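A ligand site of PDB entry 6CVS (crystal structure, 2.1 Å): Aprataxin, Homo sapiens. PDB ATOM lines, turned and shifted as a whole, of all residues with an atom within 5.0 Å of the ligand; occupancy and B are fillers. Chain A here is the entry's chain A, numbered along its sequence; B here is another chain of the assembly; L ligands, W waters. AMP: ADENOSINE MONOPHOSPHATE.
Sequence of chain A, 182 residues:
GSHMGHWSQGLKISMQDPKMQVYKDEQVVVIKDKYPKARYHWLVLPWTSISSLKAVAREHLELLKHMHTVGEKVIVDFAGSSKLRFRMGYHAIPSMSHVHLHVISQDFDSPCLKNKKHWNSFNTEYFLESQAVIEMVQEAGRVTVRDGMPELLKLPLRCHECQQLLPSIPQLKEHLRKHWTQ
Residues that only touch the ligand: Leu 11 (3.3 Å), Tyr 35 (3.4 Å), His 41 (3.5 Å), Leu 43 (3.6 Å), Pro 94 (3.7 Å), DG 1 of chain B (3.9 Å) and Gly 10 (3.97 Å). Hydrophobic or aromatic side chains within 4 Å of the ligand: Leu 11, Tyr 35, His 41, Leu 43, His 91, Pro 94, Met 96, His 100 and His 102.
Water W4 lies within hydrogen-bond range of OP1 of DG 1 of chain B, OG of Ser 95 and O1P of the ligand. Water W3 bridges NZ of Lys 37 and O3' of the ligand. Water W2 lies within hydrogen-bond range of O2P of the ligand, N of His 91 and NE2 of His 100. Water W1 lies within hydrogen-bond range of O of Gly 10 (3.0 Å), N6 of the ligand (3.2 Å) and OG of Ser 14 (3.3 Å).
N of Tyr 35 sits at hydrogen-bond distance from OD1 of Asp 33. O of His 41 lies within hydrogen-bond range of N of Asp 33 (2.9 Å). The side-chain sulfur of Met 20 is in hydrogen-bond range of the side-chain hydroxyl of Ser 14, at 3.4 Å. ND1 of His 102 lies within hydrogen-bond range of NE2 of His 41, at 3.0 Å. NZ of Lys 37 is in hydrogen-bond range of O of Tyr 35, at 2.9 Å. The backbone NH (N) of Lys 37 sits at hydrogen-bond distance from a ring nitrogen (ND1) of His 41 (3.1 Å). NZ of Lys 37 is in salt-bridge range of OP1 of DT 2 of chain B. N of Leu 43 is in hydrogen-bond range of O of Ile 31.
The side-chain carboxylate (OD2) of Asp 33 is in hydrogen-bond range of an oxygen (O3') of the ligand. NE2 of His 100 lies within hydrogen-bond range of O2P of the ligand, at 2.5 Å. O1P of the ligand lies within hydrogen-bond range of ND1 of His 91, at 2.6 Å. The side-chain hydroxyl (OG) of Ser 14 sits at hydrogen-bond distance from a nitrogen (N1) of the ligand, at 2.7 Å. O3P of the ligand sits at hydrogen-bond distance from N of Ser 95. A ring nitrogen (NE2) of His 102 is in hydrogen-bond range of an oxygen (O2P) of the ligand (2.8 Å). An oxygen (O3P) of the ligand lies within hydrogen-bond range of the backbone NH (N) of Met 96 (2.9 Å). The backbone NH (N) of Lys 34 sits at hydrogen-bond distance from a nitrogen (N3) of the ligand, 3.4 Å away. The side-chain amino group (NZ) of Lys 37 is in hydrogen-bond range of an oxygen (O2') of the ligand, 3.4 Å away.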
ATOM      1  N   GLY A  10       4.896  -6.664  21.161  1.00  0.00           N
ATOM      2  CA  GLY A  10       4.939  -5.805  19.990  1.00  0.00           C
ATOM      3  C   GLY A  10       6.086  -4.820  19.985  1.00  0.00           C
ATOM      4  O   GLY A  10       6.578  -4.444  18.919  1.00  0.00           O
ATOM      5  N   LEU A  11       6.527  -4.363  21.170  1.00  0.00           N
ATOM      6  CA  LEU A  11       7.604  -3.387  21.214  1.00  0.00           C
ATOM      7  C   LEU A  11       8.916  -3.968  20.693  1.00  0.00           C
ATOM      8  O   LEU A  11       9.717  -3.250  20.095  1.00  0.00           O
ATOM      9  CB  LEU A  11       7.802  -2.874  22.645  1.00  0.00           C
ATOM     10  CG  LEU A  11       6.649  -2.091  23.285  1.00  0.00           C
ATOM     11  CD1 LEU A  11       7.093  -1.533  24.617  1.00  0.00           C
ATOM     12  CD2 LEU A  11       6.141  -0.980  22.375  1.00  0.00           C
ATOM     13  N   SER A  14       8.617  -3.211  17.026  1.00  0.00           N
ATOM     14  CA  SER A  14       8.683  -1.801  16.658  1.00  0.00           C
ATOM     15  C   SER A  14      10.090  -1.229  16.868  1.00  0.00           C
ATOM     16  O   SER A  14      10.571  -0.438  16.050  1.00  0.00           O
ATOM     17  CB  SER A  14       7.652  -1.002  17.445  1.00  0.00           C
ATOM     18  OG  SER A  14       6.334  -1.380  17.094  1.00  0.00           O
ATOM     19  N   MET A  20       9.971   3.600  12.459  1.00  0.00           N
ATOM     20  CA  MET A  20       9.520   4.060  13.761  1.00  0.00           C
ATOM     21  C   MET A  20      10.638   4.629  14.614  1.00  0.00           C
ATOM     22  O   MET A  20      10.352   5.282  15.617  1.00  0.00           O
ATOM     23  CB  MET A  20       8.839   2.914  14.505  1.00  0.00           C
ATOM     24  CG  MET A  20       7.599   2.376  13.815  1.00  0.00           C
ATOM     25  SD  MET A  20       6.815   1.063  14.765  1.00  0.00           S
ATOM     26  CE  MET A  20       5.342   0.760  13.784  1.00  0.00           C
ATOM     27  N   ILE A  31      11.645   5.288  19.726  1.00  0.00           N
ATOM     28  CA  ILE A  31      10.634   5.105  18.690  1.00  0.00           C
ATOM     29  C   ILE A  31       9.436   5.981  19.023  1.00  0.00           C
ATOM     30  O   ILE A  31       9.198   6.361  20.171  1.00  0.00           O
ATOM     31  CB  ILE A  31      10.194   3.636  18.542  1.00  0.00           C
ATOM     32  CG1 ILE A  31       9.617   3.104  19.855  1.00  0.00           C
ATOM     33  CG2 ILE A  31      11.360   2.776  18.081  1.00  0.00           C
ATOM     34  CD1 ILE A  31       8.845   1.807  19.698  1.00  0.00           C
ATOM     35  N   LYS A  32       8.678   6.318  17.974  1.00  0.00           N
ATOM     36  CA  LYS A  32       7.374   6.920  18.176  1.00  0.00           C
ATOM     37  C   LYS A  32       6.430   5.886  18.782  1.00  0.00           C
ATOM     38  O   LYS A  32       6.437   4.719  18.389  1.00  0.00           O
ATOM     39  CB  LYS A  32       6.812   7.431  16.847  1.00  0.00           C
ATOM     40  CG  LYS A  32       7.712   8.435  16.146  1.00  0.00           C
ATOM     41  CD  LYS A  32       7.045   9.049  14.922  1.00  0.00           C
ATOM     42  CE  LYS A  32       6.779   8.016  13.838  1.00  0.00           C
ATOM     43  NZ  LYS A  32       6.180   8.628  12.616  1.00  0.00           N
ATOM     44  N   ASP A  33       5.646   6.324  19.758  1.00  0.00           N
ATOM     45  CA  ASP A  33       4.584   5.470  20.289  1.00  0.00           C
ATOM     46  C   ASP A  33       3.563   5.197  19.183  1.00  0.00           C
ATOM     47  O   ASP A  33       3.118   6.120  18.504  1.00  0.00           O
ATOM     48  CB  ASP A  33       3.923   6.134  21.489  1.00  0.00           C
ATOM     49  CG  ASP A  33       3.050   5.187  22.283  1.00  0.00           C
ATOM     50  OD1 ASP A  33       1.921   4.903  21.839  1.00  0.00           O
ATOM     51  OD2 ASP A  33       3.488   4.739  23.363  1.00  0.00           O
ATOM     52  N   LYS A  34       3.218   3.918  19.007  1.00  0.00           N
ATOM     53  CA  LYS A  34       2.301   3.554  17.928  1.00  0.00           C
ATOM     54  C   LYS A  34       0.914   4.151  18.154  1.00  0.00           C
ATOM     55  O   LYS A  34       0.169   4.369  17.195  1.00  0.00           O
ATOM     56  CB  LYS A  34       2.216   2.030  17.814  1.00  0.00           C
ATOM     57  CG  LYS A  34       1.420   1.532  16.626  1.00  0.00           C
ATOM     58  CD  LYS A  34       1.607   0.031  16.438  1.00  0.00           C
ATOM     59  CE  LYS A  34       0.919  -0.481  15.191  1.00  0.00           C
ATOM     60  NZ  LYS A  34       1.018  -1.967  15.081  1.00  0.00           N
ATOM     61  N   TYR A  35       0.553   4.407  19.409  1.00  0.00           N
ATOM     62  CA  TYR A  35      -0.757   4.959  19.758  1.00  0.00           C
ATOM     63  C   TYR A  35      -0.541   6.156  20.668  1.00  0.00           C
ATOM     64  O   TYR A  35      -0.867   6.124  21.861  1.00  0.00           O
ATOM     65  CB  TYR A  35      -1.621   3.889  20.434  1.00  0.00           C
ATOM     66  CG  TYR A  35      -1.651   2.589  19.669  1.00  0.00           C
ATOM     67  CD1 TYR A  35      -2.552   2.394  18.641  1.00  0.00           C
ATOM     68  CD2 TYR A  35      -0.764   1.561  19.954  1.00  0.00           C
ATOM     69  CE1 TYR A  35      -2.594   1.214  17.928  1.00  0.00           C
ATOM     70  CE2 TYR A  35      -0.793   0.369  19.246  1.00  0.00           C
ATOM     71  CZ  TYR A  35      -1.706   0.212  18.231  1.00  0.00           C
ATOM     72  OH  TYR A  35      -1.749  -0.968  17.518  1.00  0.00           O
ATOM     73  N   LYS A  37      -0.508   9.216  23.032  1.00  0.00           N
ATOM     74  CA  LYS A  37      -1.512   9.773  23.917  1.00  0.00           C
ATOM     75  C   LYS A  37      -1.403  11.284  24.047  1.00  0.00           C
ATOM     76  O   LYS A  37      -2.137  11.886  24.839  1.00  0.00           O
ATOM     77  CB  LYS A  37      -1.407   9.119  25.307  1.00  0.00           C
ATOM     78  CG  LYS A  37      -1.620   7.605  25.292  1.00  0.00           C
ATOM     79  CD  LYS A  37      -2.876   7.226  24.505  1.00  0.00           C
ATOM     80  CE  LYS A  37      -3.239   5.766  24.672  1.00  0.00           C
ATOM     81  NZ  LYS A  37      -2.201   4.874  24.079  1.00  0.00           N
ATOM     82  N   HIS A  41       4.859  11.774  21.780  1.00  0.00           N
ATOM     83  CA  HIS A  41       4.873  10.603  22.647  1.00  0.00           C
ATOM     84  C   HIS A  41       5.869   9.606  22.068  1.00  0.00           C
ATOM     85  O   HIS A  41       5.565   8.926  21.087  1.00  0.00           O
ATOM     86  CB  HIS A  41       3.486  10.004  22.779  1.00  0.00           C
ATOM     87  CG  HIS A  41       3.379   8.961  23.845  1.00  0.00           C
ATOM     88  ND1 HIS A  41       2.182   8.382  24.208  1.00  0.00           N
ATOM     89  CD2 HIS A  41       4.324   8.404  24.637  1.00  0.00           C
ATOM     90  CE1 HIS A  41       2.400   7.505  25.175  1.00  0.00           C
ATOM     91  NE2 HIS A  41       3.685   7.497  25.456  1.00  0.00           N
ATOM     92  N   LEU A  43       8.911   6.443  23.011  1.00  0.00           N
ATOM     93  CA  LEU A  43       9.342   5.414  23.947  1.00  0.00           C
ATOM     94  C   LEU A  43      10.839   5.204  23.776  1.00  0.00           C
ATOM     95  O   LEU A  43      11.310   4.958  22.651  1.00  0.00           O
ATOM     96  CB  LEU A  43       8.598   4.098  23.711  1.00  0.00           C
ATOM     97  CG  LEU A  43       7.094   4.146  23.893  1.00  0.00           C
ATOM     98  CD1 LEU A  43       6.495   2.821  23.451  1.00  0.00           C
ATOM     99  CD2 LEU A  43       6.732   4.456  25.338  1.00  0.00           C
ATOM    100  N   HIS A  91       5.097   3.302  33.584  1.00  0.00           N
ATOM    101  CA  HIS A  91       3.859   2.828  34.177  1.00  0.00           C
ATOM    102  C   HIS A  91       4.156   1.793  35.257  1.00  0.00           C
ATOM    103  O   HIS A  91       4.922   0.853  35.031  1.00  0.00           O
ATOM    104  CB  HIS A  91       2.946   2.236  33.107  1.00  0.00           C
ATOM    105  CG  HIS A  91       2.252   3.262  32.266  1.00  0.00           C
ATOM    106  ND1 HIS A  91       1.684   2.961  31.045  1.00  0.00           N
ATOM    107  CD2 HIS A  91       2.012   4.573  32.479  1.00  0.00           C
ATOM    108  CE1 HIS A  91       1.133   4.050  30.541  1.00  0.00           C
ATOM    109  NE2 HIS A  91       1.324   5.049  31.389  1.00  0.00           N
ATOM    110  N   ILE A  93       2.579  -0.613  36.411  1.00  0.00           N
ATOM    111  CA  ILE A  93       2.292  -1.961  35.936  1.00  0.00           C
ATOM    112  C   ILE A  93       2.178  -1.868  34.413  1.00  0.00           C
ATOM    113  O   ILE A  93       1.163  -1.389  33.903  1.00  0.00           O
ATOM    114  CB  ILE A  93       1.000  -2.521  36.544  1.00  0.00           C
ATOM    115  CG1 ILE A  93       1.099  -2.535  38.072  1.00  0.00           C
ATOM    116  CG2 ILE A  93       0.739  -3.934  36.004  1.00  0.00           C
ATOM    117  CD1 ILE A  93      -0.209  -2.889  38.754  1.00  0.00           C
ATOM    118  N   PRO A  94       3.201  -2.282  33.657  1.00  0.00           N
ATOM    119  CA  PRO A  94       3.115  -2.161  32.196  1.00  0.00           C
ATOM    120  C   PRO A  94       2.296  -3.288  31.592  1.00  0.00           C
ATOM    121  O   PRO A  94       2.044  -4.320  32.212  1.00  0.00           O
ATOM    122  CB  PRO A  94       4.585  -2.249  31.768  1.00  0.00           C
ATOM    123  CG  PRO A  94       5.196  -3.148  32.782  1.00  0.00           C
ATOM    124  CD  PRO A  94       4.475  -2.867  34.088  1.00  0.00           C
ATOM    125  N   SER A  95       1.873  -3.050  30.357  1.00  0.00           N
ATOM    126  CA  SER A  95       1.230  -4.084  29.554  1.00  0.00           C
ATOM    127  C   SER A  95       2.193  -4.722  28.561  1.00  0.00           C
ATOM    128  O   SER A  95       2.158  -5.938  28.373  1.00  0.00           O
ATOM    129  CB  SER A  95       0.044  -3.490  28.783  1.00  0.00           C
ATOM    130  OG  SER A  95      -0.927  -2.971  29.675  1.00  0.00           O
ATOM    131  N   MET A  96       3.051  -3.912  27.955  1.00  0.00           N
ATOM    132  CA  MET A  96       3.994  -4.362  26.941  1.00  0.00           C
ATOM    133  C   MET A  96       5.320  -4.751  27.567  1.00  0.00           C
ATOM    134  O   MET A  96       5.841  -4.046  28.437  1.00  0.00           O
ATOM    135  CB  MET A  96       4.209  -3.265  25.894  1.00  0.00           C
ATOM    136  CG  MET A  96       2.922  -2.733  25.276  1.00  0.00           C
ATOM    137  SD  MET A  96       2.120  -3.921  24.184  1.00  0.00           S
ATOM    138  CE  MET A  96       3.237  -3.883  22.765  1.00  0.00           C
ATOM    139  N   HIS A 100      10.629   0.232  28.899  1.00  0.00           N
ATOM    140  CA  HIS A 100      10.510   1.383  28.009  1.00  0.00           C
ATOM    141  C   HIS A 100      10.141   2.622  28.806  1.00  0.00           C
ATOM    142  O   HIS A 100       9.260   2.582  29.665  1.00  0.00           O
ATOM    143  CB  HIS A 100       9.459   1.116  26.924  1.00  0.00           C
ATOM    144  CG  HIS A 100       8.158   0.624  27.460  1.00  0.00           C
ATOM    145  ND1 HIS A 100       7.905  -0.702  27.714  1.00  0.00           N
ATOM    146  CD2 HIS A 100       7.023   1.288  27.792  1.00  0.00           C
ATOM    147  CE1 HIS A 100       6.680  -0.844  28.168  1.00  0.00           C
ATOM    148  NE2 HIS A 100       6.118   0.351  28.236  1.00  0.00           N
ATOM    149  N   HIS A 102       8.517   6.236  28.886  1.00  0.00           N
ATOM    150  CA  HIS A 102       7.595   7.148  28.227  1.00  0.00           C
ATOM    151  C   HIS A 102       8.152   8.561  28.236  1.00  0.00           C
ATOM    152  O   HIS A 102       8.666   9.041  29.259  1.00  0.00           O
ATOM    153  CB  HIS A 102       6.236   7.143  28.935  1.00  0.00           C
ATOM    154  CG  HIS A 102       5.463   5.868  28.758  1.00  0.00           C
ATOM    155  ND1 HIS A 102       4.558   5.686  27.735  1.00  0.00           N
ATOM    156  CD2 HIS A 102       5.444   4.724  29.487  1.00  0.00           C
ATOM    157  CE1 HIS A 102       4.031   4.482  27.832  1.00  0.00           C
ATOM    158  NE2 HIS A 102       4.549   3.875  28.885  1.00  0.00           N
ATOM    159  N   PHE A 122      -1.248   8.051  33.187  1.00  0.00           N
ATOM    160  CA  PHE A 122      -0.289   9.121  33.038  1.00  0.00           C
ATOM    161  C   PHE A 122      -0.486  10.257  34.045  1.00  0.00           C
ATOM    162  O   PHE A 122       0.328  11.179  34.074  1.00  0.00           O
ATOM    163  CB  PHE A 122      -0.358   9.710  31.624  1.00  0.00           C
ATOM    164  CG  PHE A 122       0.164   8.774  30.558  1.00  0.00           C
ATOM    165  CD1 PHE A 122       1.519   8.661  30.327  1.00  0.00           C
ATOM    166  CD2 PHE A 122      -0.716   8.025  29.788  1.00  0.00           C
ATOM    167  CE1 PHE A 122       2.005   7.807  29.356  1.00  0.00           C
ATOM    168  CE2 PHE A 122      -0.240   7.171  28.808  1.00  0.00           C
ATOM    169  CZ  PHE A 122       1.115   7.066  28.597  1.00  0.00           C
ATOM    170  OP3  DG B   1      -4.135   1.330  27.477  1.00  0.00           O
ATOM    171  P    DG B   1      -3.533   0.164  28.413  1.00  0.00           P
ATOM    172  OP1  DG B   1      -2.701   0.798  29.463  1.00  0.00           O
ATOM    173  OP2  DG B   1      -4.654  -0.707  28.813  1.00  0.00           O
ATOM    174  O5'  DG B   1      -2.570  -0.721  27.504  1.00  0.00           O
ATOM    175  C5'  DG B   1      -1.402  -0.151  26.950  1.00  0.00           C
ATOM    176  C4'  DG B   1      -1.157  -0.681  25.555  1.00  0.00           C
ATOM    177  O4'  DG B   1      -0.803  -2.079  25.630  1.00  0.00           O
ATOM    178  C3'  DG B   1      -2.371  -0.613  24.640  1.00  0.00           C
ATOM    179  O3'  DG B   1      -2.440   0.631  23.969  1.00  0.00           O
ATOM    180  C2'  DG B   1      -2.125  -1.776  23.695  1.00  0.00           C
ATOM    181  C1'  DG B   1      -1.460  -2.807  24.596  1.00  0.00           C
ATOM    182  N9   DG B   1      -2.399  -3.735  25.215  1.00  0.00           N
ATOM    183  C8   DG B   1      -2.697  -3.864  26.541  1.00  0.00           C
ATOM    184  N7   DG B   1      -3.593  -4.788  26.786  1.00  0.00           N
ATOM    185  C5   DG B   1      -3.897  -5.304  25.543  1.00  0.00           C
ATOM    186  C6   DG B   1      -4.787  -6.328  25.170  1.00  0.00           C
ATOM    187  O6   DG B   1      -5.528  -7.013  25.896  1.00  0.00           O
ATOM    188  N1   DG B   1      -4.805  -6.532  23.794  1.00  0.00           N
ATOM    189  C2   DG B   1      -4.036  -5.833  22.888  1.00  0.00           C
ATOM    190  N2   DG B   1      -4.176  -6.170  21.598  1.00  0.00           N
ATOM    191  N3   DG B   1      -3.187  -4.874  23.224  1.00  0.00           N
ATOM    192  C4   DG B   1      -3.174  -4.664  24.553  1.00  0.00           C
ATOM    193  P    DT B   2      -3.876   1.275  23.620  1.00  0.00           P
ATOM    194  OP1  DT B   2      -3.636   2.629  23.077  1.00  0.00           O
ATOM    195  OP2  DT B   2      -4.745   1.094  24.801  1.00  0.00           O
ATOM    196  O5'  DT B   2      -4.432   0.318  22.457  1.00  0.00           O
ATOM    197  C5'  DT B   2      -3.686   0.149  21.265  1.00  0.00           C
ATOM    198  C4'  DT B   2      -4.387  -0.799  20.307  1.00  0.00           C
ATOM    199  O4'  DT B   2      -4.657  -2.060  20.990  1.00  0.00           O
ATOM    200  C3'  DT B   2      -5.731  -0.307  19.778  1.00  0.00           C
ATOM    201  O3'  DT B   2      -5.846  -0.537  18.381  1.00  0.00           O
ATOM    202  C2'  DT B   2      -6.760  -1.093  20.587  1.00  0.00           C
ATOM    203  C1'  DT B   2      -6.026  -2.384  20.919  1.00  0.00           C
ATOM    204  N1   DT B   2      -6.448  -2.983  22.217  1.00  0.00           N
ATOM    205  C2   DT B   2      -7.193  -4.134  22.212  1.00  0.00           C
ATOM    206  O2   DT B   2      -7.556  -4.696  21.190  1.00  0.00           O
ATOM    207  N3   DT B   2      -7.530  -4.616  23.453  1.00  0.00           N
ATOM    208  C4   DT B   2      -7.189  -4.065  24.678  1.00  0.00           C
ATOM    209  O4   DT B   2      -7.542  -4.570  25.734  1.00  0.00           O
ATOM    210  C5   DT B   2      -6.395  -2.860  24.613  1.00  0.00           C
ATOM    211  C7   DT B   2      -5.964  -2.174  25.876  1.00  0.00           C
ATOM    212  C6   DT B   2      -6.074  -2.384  23.398  1.00  0.00           C
HETATM  213  P   AMP L   1       2.775   0.366  28.977  1.00  0.00           P
HETATM  214  O1P AMP L   1       1.637   0.503  30.103  1.00  0.00           O
HETATM  215  O2P AMP L   1       3.993   1.135  29.394  1.00  0.00           O
HETATM  216  O3P AMP L   1       2.913  -1.102  28.638  1.00  0.00           O
HETATM  217  O5' AMP L   1       2.202   1.072  27.687  1.00  0.00           O
HETATM  218  C5' AMP L   1       2.543   0.602  26.395  1.00  0.00           C
HETATM  219  C4' AMP L   1       2.831   1.760  25.475  1.00  0.00           C
HETATM  220  O4' AMP L   1       3.332   1.264  24.213  1.00  0.00           O
HETATM  221  C3' AMP L   1       1.616   2.623  25.162  1.00  0.00           C
HETATM  222  O3' AMP L   1       2.013   4.001  25.114  1.00  0.00           O
HETATM  223  C2' AMP L   1       1.189   2.137  23.771  1.00  0.00           C
HETATM  224  O2' AMP L   1       0.530   3.101  22.986  1.00  0.00           O
HETATM  225  C1' AMP L   1       2.528   1.716  23.149  1.00  0.00           C
HETATM  226  N9  AMP L   1       2.448   0.619  22.191  1.00  0.00           N
HETATM  227  C8  AMP L   1       1.565  -0.442  22.203  1.00  0.00           C
HETATM  228  N7  AMP L   1       1.780  -1.294  21.185  1.00  0.00           N
HETATM  229  C5  AMP L   1       2.859  -0.754  20.510  1.00  0.00           C
HETATM  230  C6  AMP L   1       3.560  -1.158  19.367  1.00  0.00           C
HETATM  231  N6  AMP L   1       3.264  -2.272  18.666  1.00  0.00           N
HETATM  232  N1  AMP L   1       4.585  -0.390  18.944  1.00  0.00           N
HETATM  233  C2  AMP L   1       4.904   0.723  19.621  1.00  0.00           C
HETATM  234  N3  AMP L   1       4.302   1.196  20.705  1.00  0.00           N
HETATM  235  C4  AMP L   1       3.273   0.421  21.120  1.00  0.00           C
HETATM  236  O   HOH W   1       4.700  -4.189  16.531  1.00  0.00           O
HETATM  237  O   HOH W   2       6.425   1.651  31.193  1.00  0.00           O
HETATM  238  O   HOH W   3      -0.499   4.768  26.331  1.00  0.00           O
HETATM  239  O   HOH W   4      -0.757  -0.466  30.272  1.00  0.00           O
